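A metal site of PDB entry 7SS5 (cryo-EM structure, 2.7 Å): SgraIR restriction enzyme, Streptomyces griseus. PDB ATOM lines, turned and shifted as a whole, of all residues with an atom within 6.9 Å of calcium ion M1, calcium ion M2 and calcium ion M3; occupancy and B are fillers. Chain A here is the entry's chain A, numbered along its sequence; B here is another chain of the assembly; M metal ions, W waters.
The backbone NH of Leu 150 is in hydrogen-bond range of the backbone carbonyl oxygen of Asp 188, 3.1 Å away.
O4' of DC 19 of chain B is in hydrogen-bond range of the guanidinium group (NH2) of Arg 152, 3.5 Å away.
O of Glu 103 is in hydrogen-bond range of OG of Ser 107 (3.2 Å).
Within 4 Å of calcium ion M1: Glu 103, Asn 149, Leu 150 and Asp 188.
Three residues have an atom within 4 Å of calcium ion M2: Glu 103, Asp 188 and DC 19 of chain B.
The nearest printed residue that does not touch calcium ion M2 is DA 18 of chain B (4.9 Å).
Four residues have an atom within 4 Å of calcium ion M3: Glu 103, Asp 188, Phe 241 and DC 19 of chain B.
Along chain A the residues within 4 Å of calcium ion M3 span positions 103 to 241.
Calcium ion M1 is bound by O of Leu 150 (2.3 Å).
The side-chain carboxylate (OE2) of Glu 103 binds calcium ion M1, at 2.4 Å.
OD1 of Asn 149 is bound to calcium ion M1 (2.8 Å).
Slightly farther from calcium ion M1 lies water W4 (2.9 Å).
Calcium ion M2 is bound by OP1 of DC 19 of chain B, at 2.5 Å.
Water W2 is bound to calcium ion M2 (2.5 Å).
Calcium ion M2 is bound by the side-chain carboxylate (OD1) of Asp 188 (2.6 Å).
The side-chain carboxylate (OE1) of Glu 103 is bound to calcium ion M2 (2.6 Å).
Calcium ion M2 has four donor atoms within binding distance.
Calcium ion M3 is bound by OP2 of DC 19 of chain B (2.4 Å), water W3 (2.4 Å), water W1 (2.4 Å), O of Phe 241 (2.5 Å) and OD2 of Asp 188 (2.6 Å).
Slightly farther from calcium ion M3 lies water W5 (3.0 Å).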
ATOM      1  N   GLY A  99     -12.280  30.256  22.756  1.00  0.00           N
ATOM      2  CA  GLY A  99     -11.780  30.125  21.396  1.00  0.00           C
ATOM      3  C   GLY A  99     -12.398  28.942  20.665  1.00  0.00           C
ATOM      4  O   GLY A  99     -12.799  29.063  19.497  1.00  0.00           O
ATOM      5  N   ASP A 100     -12.490  27.795  21.337  1.00  0.00           N
ATOM      6  CA  ASP A 100     -13.106  26.632  20.699  1.00  0.00           C
ATOM      7  C   ASP A 100     -14.570  26.882  20.370  1.00  0.00           C
ATOM      8  O   ASP A 100     -15.048  26.485  19.292  1.00  0.00           O
ATOM      9  CB  ASP A 100     -12.966  25.412  21.611  1.00  0.00           C
ATOM     10  CG  ASP A 100     -11.562  24.825  21.590  1.00  0.00           C
ATOM     11  OD1 ASP A 100     -10.691  25.399  20.895  1.00  0.00           O
ATOM     12  OD2 ASP A 100     -11.338  23.805  22.257  1.00  0.00           O
ATOM     13  N   PHE A 102     -16.008  29.815  19.758  1.00  0.00           N
ATOM     14  CA  PHE A 102     -16.026  30.725  18.622  1.00  0.00           C
ATOM     15  C   PHE A 102     -15.844  29.974  17.313  1.00  0.00           C
ATOM     16  O   PHE A 102     -16.618  30.143  16.367  1.00  0.00           O
ATOM     17  CB  PHE A 102     -14.941  31.783  18.802  1.00  0.00           C
ATOM     18  CG  PHE A 102     -14.809  32.737  17.645  1.00  0.00           C
ATOM     19  CD1 PHE A 102     -15.903  33.411  17.140  1.00  0.00           C
ATOM     20  CD2 PHE A 102     -13.569  32.968  17.061  1.00  0.00           C
ATOM     21  CE1 PHE A 102     -15.775  34.282  16.075  1.00  0.00           C
ATOM     22  CE2 PHE A 102     -13.432  33.842  15.999  1.00  0.00           C
ATOM     23  CZ  PHE A 102     -14.538  34.503  15.508  1.00  0.00           C
ATOM     24  N   GLU A 103     -14.831  29.094  17.272  1.00  0.00           N
ATOM     25  CA  GLU A 103     -14.576  28.325  16.058  1.00  0.00           C
ATOM     26  C   GLU A 103     -15.786  27.466  15.679  1.00  0.00           C
ATOM     27  O   GLU A 103     -16.240  27.502  14.525  1.00  0.00           O
ATOM     28  CB  GLU A 103     -13.343  27.444  16.249  1.00  0.00           C
ATOM     29  CG  GLU A 103     -12.691  26.994  14.955  1.00  0.00           C
ATOM     30  CD  GLU A 103     -11.781  25.802  15.139  1.00  0.00           C
ATOM     31  OE1 GLU A 103     -10.884  25.859  16.012  1.00  0.00           O
ATOM     32  OE2 GLU A 103     -11.950  24.805  14.411  1.00  0.00           O
ATOM     33  N   SER A 107     -18.288  27.850  12.418  1.00  0.00           N
ATOM     34  CA  SER A 107     -18.380  26.733  11.485  1.00  0.00           C
ATOM     35  C   SER A 107     -19.826  26.310  11.267  1.00  0.00           C
ATOM     36  O   SER A 107     -20.236  26.025  10.136  1.00  0.00           O
ATOM     37  CB  SER A 107     -17.551  25.551  11.997  1.00  0.00           C
ATOM     38  OG  SER A 107     -16.162  25.813  11.861  1.00  0.00           O
ATOM     39  N   LEU A 148     -16.160  22.077   5.703  1.00  0.00           N
ATOM     40  CA  LEU A 148     -15.547  21.052   6.546  1.00  0.00           C
ATOM     41  C   LEU A 148     -14.807  21.731   7.698  1.00  0.00           C
ATOM     42  O   LEU A 148     -13.939  22.582   7.460  1.00  0.00           O
ATOM     43  CB  LEU A 148     -14.591  20.182   5.737  1.00  0.00           C
ATOM     44  CG  LEU A 148     -15.143  19.536   4.473  1.00  0.00           C
ATOM     45  CD1 LEU A 148     -14.111  18.602   3.860  1.00  0.00           C
ATOM     46  CD2 LEU A 148     -16.436  18.792   4.772  1.00  0.00           C
ATOM     47  N   ASN A 149     -15.169  21.363   8.916  1.00  0.00           N
ATOM     48  CA  ASN A 149     -14.414  21.764  10.098  1.00  0.00           C
ATOM     49  C   ASN A 149     -13.404  20.671  10.400  1.00  0.00           C
ATOM     50  O   ASN A 149     -13.781  19.527  10.680  1.00  0.00           O
ATOM     51  CB  ASN A 149     -15.353  21.993  11.291  1.00  0.00           C
ATOM     52  CG  ASN A 149     -14.608  22.144  12.598  1.00  0.00           C
ATOM     53  OD1 ASN A 149     -13.903  23.119  12.821  1.00  0.00           O
ATOM     54  ND2 ASN A 149     -14.756  21.152  13.476  1.00  0.00           N
ATOM     55  N   LEU A 150     -12.133  21.014  10.348  1.00  0.00           N
ATOM     56  CA  LEU A 150     -11.131  19.963  10.418  1.00  0.00           C
ATOM     57  C   LEU A 150     -10.716  19.704  11.869  1.00  0.00           C
ATOM     58  O   LEU A 150     -10.790  20.601  12.709  1.00  0.00           O
ATOM     59  CB  LEU A 150      -9.892  20.345   9.594  1.00  0.00           C
ATOM     60  CG  LEU A 150     -10.175  20.761   8.148  1.00  0.00           C
ATOM     61  CD1 LEU A 150      -8.999  21.525   7.564  1.00  0.00           C
ATOM     62  CD2 LEU A 150     -10.505  19.538   7.290  1.00  0.00           C
ATOM     63  N   PRO A 151     -10.289  18.473  12.173  1.00  0.00           N
ATOM     64  CA  PRO A 151      -9.838  18.174  13.538  1.00  0.00           C
ATOM     65  C   PRO A 151      -8.546  18.887  13.906  1.00  0.00           C
ATOM     66  O   PRO A 151      -7.988  19.629  13.093  1.00  0.00           O
ATOM     67  CB  PRO A 151      -9.643  16.646  13.521  1.00  0.00           C
ATOM     68  CG  PRO A 151     -10.347  16.161  12.288  1.00  0.00           C
ATOM     69  CD  PRO A 151     -10.286  17.278  11.304  1.00  0.00           C
ATOM     70  N   ARG A 152      -8.068  18.658  15.130  1.00  0.00           N
ATOM     71  CA  ARG A 152      -6.911  19.399  15.619  1.00  0.00           C
ATOM     72  C   ARG A 152      -5.628  18.965  14.922  1.00  0.00           C
ATOM     73  O   ARG A 152      -4.807  19.807  14.545  1.00  0.00           O
ATOM     74  CB  ARG A 152      -6.782  19.235  17.135  1.00  0.00           C
ATOM     75  CG  ARG A 152      -7.863  19.950  17.918  1.00  0.00           C
ATOM     76  CD  ARG A 152      -7.540  19.996  19.399  1.00  0.00           C
ATOM     77  NE  ARG A 152      -6.941  21.265  19.793  1.00  0.00           N
ATOM     78  CZ  ARG A 152      -7.631  22.312  20.224  1.00  0.00           C
ATOM     79  NH1 ARG A 152      -8.954  22.281  20.315  1.00  0.00           N
ATOM     80  NH2 ARG A 152      -6.987  23.419  20.569  1.00  0.00           N
ATOM     81  N   THR A 186      -2.874  22.466  11.545  1.00  0.00           N
ATOM     82  CA  THR A 186      -4.069  22.262  10.738  1.00  0.00           C
ATOM     83  C   THR A 186      -4.874  23.548  10.635  1.00  0.00           C
ATOM     84  O   THR A 186      -5.166  24.171  11.669  1.00  0.00           O
ATOM     85  CB  THR A 186      -4.934  21.148  11.327  1.00  0.00           C
ATOM     86  OG1 THR A 186      -4.112  20.027  11.675  1.00  0.00           O
ATOM     87  CG2 THR A 186      -5.995  20.708  10.339  1.00  0.00           C
ATOM     88  N   PRO A 187      -5.256  23.978   9.437  1.00  0.00           N
ATOM     89  CA  PRO A 187      -6.189  25.099   9.325  1.00  0.00           C
ATOM     90  C   PRO A 187      -7.549  24.744   9.900  1.00  0.00           C
ATOM     91  O   PRO A 187      -7.943  23.578   9.945  1.00  0.00           O
ATOM     92  CB  PRO A 187      -6.275  25.359   7.811  1.00  0.00           C
ATOM     93  CG  PRO A 187      -5.696  24.153   7.169  1.00  0.00           C
ATOM     94  CD  PRO A 187      -4.757  23.521   8.136  1.00  0.00           C
ATOM     95  N   ASP A 188      -8.269  25.767  10.347  1.00  0.00           N
ATOM     96  CA  ASP A 188      -9.518  25.539  11.071  1.00  0.00           C
ATOM     97  C   ASP A 188     -10.615  25.013  10.145  1.00  0.00           C
ATOM     98  O   ASP A 188     -11.143  23.916  10.357  1.00  0.00           O
ATOM     99  CB  ASP A 188      -9.965  26.837  11.752  1.00  0.00           C
ATOM    100  CG  ASP A 188      -9.162  27.134  13.000  1.00  0.00           C
ATOM    101  OD1 ASP A 188      -8.643  26.189  13.618  1.00  0.00           O
ATOM    102  OD2 ASP A 188      -9.042  28.330  13.356  1.00  0.00           O
ATOM    103  N   LEU A 189     -10.988  25.783   9.127  1.00  0.00           N
ATOM    104  CA  LEU A 189     -12.135  25.444   8.297  1.00  0.00           C
ATOM    105  C   LEU A 189     -11.757  25.487   6.819  1.00  0.00           C
ATOM    106  O   LEU A 189     -10.970  26.343   6.397  1.00  0.00           O
ATOM    107  CB  LEU A 189     -13.294  26.416   8.575  1.00  0.00           C
ATOM    108  CG  LEU A 189     -14.598  26.241   7.790  1.00  0.00           C
ATOM    109  CD1 LEU A 189     -15.780  26.535   8.690  1.00  0.00           C
ATOM    110  CD2 LEU A 189     -14.615  27.143   6.568  1.00  0.00           C
ATOM    111  N   ALA A 240      -9.103  30.610   9.171  1.00  0.00           N
ATOM    112  CA  ALA A 240      -8.546  30.424  10.501  1.00  0.00           C
ATOM    113  C   ALA A 240      -9.224  31.382  11.474  1.00  0.00           C
ATOM    114  O   ALA A 240      -9.332  32.576  11.202  1.00  0.00           O
ATOM    115  CB  ALA A 240      -7.037  30.651  10.503  1.00  0.00           C
ATOM    116  N   PHE A 241      -9.646  30.856  12.617  1.00  0.00           N
ATOM    117  CA  PHE A 241     -10.389  31.631  13.615  1.00  0.00           C
ATOM    118  C   PHE A 241      -9.495  31.916  14.813  1.00  0.00           C
ATOM    119  O   PHE A 241      -8.814  31.013  15.320  1.00  0.00           O
ATOM    120  CB  PHE A 241     -11.638  30.886  14.071  1.00  0.00           C
ATOM    121  CG  PHE A 241     -12.658  30.695  12.998  1.00  0.00           C
ATOM    122  CD1 PHE A 241     -13.449  31.743  12.579  1.00  0.00           C
ATOM    123  CD2 PHE A 241     -12.844  29.446  12.416  1.00  0.00           C
ATOM    124  CE1 PHE A 241     -14.393  31.568  11.585  1.00  0.00           C
ATOM    125  CE2 PHE A 241     -13.785  29.259  11.428  1.00  0.00           C
ATOM    126  CZ  PHE A 241     -14.570  30.323  11.006  1.00  0.00           C
ATOM    127  N   LYS A 242      -9.487  33.166  15.263  1.00  0.00           N
ATOM    128  CA  LYS A 242      -8.777  33.567  16.473  1.00  0.00           C
ATOM    129  C   LYS A 242      -9.625  34.599  17.194  1.00  0.00           C
ATOM    130  O   LYS A 242      -9.858  35.685  16.666  1.00  0.00           O
ATOM    131  CB  LYS A 242      -7.393  34.147  16.155  1.00  0.00           C
ATOM    132  CG  LYS A 242      -6.407  33.146  15.579  1.00  0.00           C
ATOM    133  CD  LYS A 242      -5.072  33.799  15.259  1.00  0.00           C
ATOM    134  CE  LYS A 242      -3.957  33.249  16.127  1.00  0.00           C
ATOM    135  NZ  LYS A 242      -3.518  31.906  15.663  1.00  0.00           N
ATOM    136  N   ARG A 243     -10.088  34.266  18.404  1.00  0.00           N
ATOM    137  CA  ARG A 243     -11.004  35.155  19.114  1.00  0.00           C
ATOM    138  C   ARG A 243     -10.371  36.512  19.390  1.00  0.00           C
ATOM    139  O   ARG A 243     -11.058  37.534  19.355  1.00  0.00           O
ATOM    140  CB  ARG A 243     -11.471  34.506  20.412  1.00  0.00           C
ATOM    141  CG  ARG A 243     -12.867  34.945  20.861  1.00  0.00           C
ATOM    142  CD  ARG A 243     -12.969  35.041  22.370  1.00  0.00           C
ATOM    143  NE  ARG A 243     -12.105  36.088  22.914  1.00  0.00           N
ATOM    144  CZ  ARG A 243     -12.425  37.369  22.968  1.00  0.00           C
ATOM    145  NH1 ARG A 243     -13.590  37.820  22.512  1.00  0.00           N
ATOM    146  NH2 ARG A 243     -11.562  38.230  23.489  1.00  0.00           N
ATOM    147  P    DA B  18      -1.933  21.694  15.737  1.00  0.00           P
ATOM    148  OP1  DA B  18      -2.616  21.419  14.451  1.00  0.00           O
ATOM    149  OP2  DA B  18      -0.469  21.919  15.742  1.00  0.00           O
ATOM    150  O5'  DA B  18      -2.614  22.966  16.435  1.00  0.00           O
ATOM    151  C5'  DA B  18      -4.035  23.034  16.567  1.00  0.00           C
ATOM    152  C4'  DA B  18      -4.414  23.992  17.681  1.00  0.00           C
ATOM    153  O4'  DA B  18      -4.027  23.423  18.943  1.00  0.00           O
ATOM    154  C3'  DA B  18      -3.713  25.343  17.629  1.00  0.00           C
ATOM    155  O3'  DA B  18      -4.487  26.345  16.908  1.00  0.00           O
ATOM    156  C2'  DA B  18      -3.488  25.725  19.097  1.00  0.00           C
ATOM    157  C1'  DA B  18      -3.899  24.473  19.878  1.00  0.00           C
ATOM    158  N9   DA B  18      -2.919  24.077  20.893  1.00  0.00           N
ATOM    159  C8   DA B  18      -1.587  23.850  20.704  1.00  0.00           C
ATOM    160  N7   DA B  18      -0.956  23.519  21.801  1.00  0.00           N
ATOM    161  C5   DA B  18      -1.935  23.532  22.774  1.00  0.00           C
ATOM    162  C6   DA B  18      -1.912  23.276  24.152  1.00  0.00           C
ATOM    163  N6   DA B  18      -0.809  22.927  24.818  1.00  0.00           N
ATOM    164  N1   DA B  18      -3.066  23.380  24.834  1.00  0.00           N
ATOM    165  C2   DA B  18      -4.179  23.725  24.164  1.00  0.00           C
ATOM    166  N3   DA B  18      -4.329  23.992  22.876  1.00  0.00           N
ATOM    167  C4   DA B  18      -3.162  23.880  22.226  1.00  0.00           C
ATOM    168  P    DC B  19      -6.067  26.589  17.136  1.00  0.00           P
ATOM    169  OP1  DC B  19      -6.854  25.408  16.703  1.00  0.00           O
ATOM    170  OP2  DC B  19      -6.342  27.886  16.477  1.00  0.00           O
ATOM    171  O5'  DC B  19      -6.264  26.810  18.712  1.00  0.00           O
ATOM    172  C5'  DC B  19      -7.589  26.851  19.250  1.00  0.00           C
ATOM    173  C4'  DC B  19      -7.625  27.454  20.650  1.00  0.00           C
ATOM    174  O4'  DC B  19      -6.729  26.756  21.526  1.00  0.00           O
ATOM    175  C3'  DC B  19      -7.182  28.907  20.762  1.00  0.00           C
ATOM    176  O3'  DC B  19      -8.253  29.773  20.426  1.00  0.00           O
ATOM    177  C2'  DC B  19      -6.805  29.020  22.243  1.00  0.00           C
ATOM    178  C1'  DC B  19      -6.433  27.583  22.631  1.00  0.00           C
ATOM    179  N1   DC B  19      -4.999  27.414  22.989  1.00  0.00           N
ATOM    180  C2   DC B  19      -4.627  27.319  24.329  1.00  0.00           C
ATOM    181  O2   DC B  19      -5.492  27.369  25.201  1.00  0.00           O
ATOM    182  N3   DC B  19      -3.311  27.162  24.628  1.00  0.00           N
ATOM    183  C4   DC B  19      -2.402  27.119  23.662  1.00  0.00           C
ATOM    184  N4   DC B  19      -1.127  26.968  24.005  1.00  0.00           N
ATOM    185  C5   DC B  19      -2.765  27.220  22.292  1.00  0.00           C
ATOM    186  C6   DC B  19      -4.061  27.371  22.005  1.00  0.00           C
ATOM    187  P    DC B  20      -7.975  31.303  20.023  1.00  0.00           P
ATOM    188  OP1  DC B  20      -9.213  31.856  19.450  1.00  0.00           O
ATOM    189  OP2  DC B  20      -6.718  31.331  19.235  1.00  0.00           O
ATOM    190  O5'  DC B  20      -7.682  32.029  21.418  1.00  0.00           O
ATOM    191  C5'  DC B  20      -8.723  32.144  22.392  1.00  0.00           C
ATOM    192  C4'  DC B  20      -8.174  32.691  23.704  1.00  0.00           C
ATOM    193  O4'  DC B  20      -7.037  31.896  24.125  1.00  0.00           O
ATOM    194  C3'  DC B  20      -7.684  34.144  23.662  1.00  0.00           C
ATOM    195  O3'  DC B  20      -7.999  34.787  24.888  1.00  0.00           O
ATOM    196  C2'  DC B  20      -6.180  33.975  23.499  1.00  0.00           C
ATOM    197  C1'  DC B  20      -5.934  32.743  24.352  1.00  0.00           C
ATOM    198  N1   DC B  20      -4.683  32.014  24.006  1.00  0.00           N
ATOM    199  C2   DC B  20      -3.741  31.746  24.994  1.00  0.00           C
ATOM    200  O2   DC B  20      -3.952  32.119  26.154  1.00  0.00           O
ATOM    201  N3   DC B  20      -2.605  31.072  24.660  1.00  0.00           N
ATOM    202  C4   DC B  20      -2.419  30.681  23.404  1.00  0.00           C
ATOM    203  N4   DC B  20      -1.283  30.023  23.114  1.00  0.00           N
ATOM    204  C5   DC B  20      -3.366  30.941  22.376  1.00  0.00           C
ATOM    205  C6   DC B  20      -4.477  31.601  22.718  1.00  0.00           C
HETATM  206 CA    CA M   1     -11.128  22.814  13.332  1.00  0.00          CA
HETATM  207 CA    CA M   2      -8.747  24.397  15.455  1.00  0.00          CA
HETATM  208 CA    CA M   3      -8.569  28.617  15.889  1.00  0.00          CA
HETATM  209  O   HOH W   1     -10.013  29.139  17.779  1.00  0.00           O
HETATM  210  O   HOH W   2      -6.759  24.863  13.966  1.00  0.00           O
HETATM  211  O   HOH W   3      -6.953  29.483  14.298  1.00  0.00           O
HETATM  212  O   HOH W   4     -11.567  21.083  15.670  1.00  0.00           O
HETATM  213  O   HOH W   5      -6.226  30.160  17.034  1.00  0.00           O
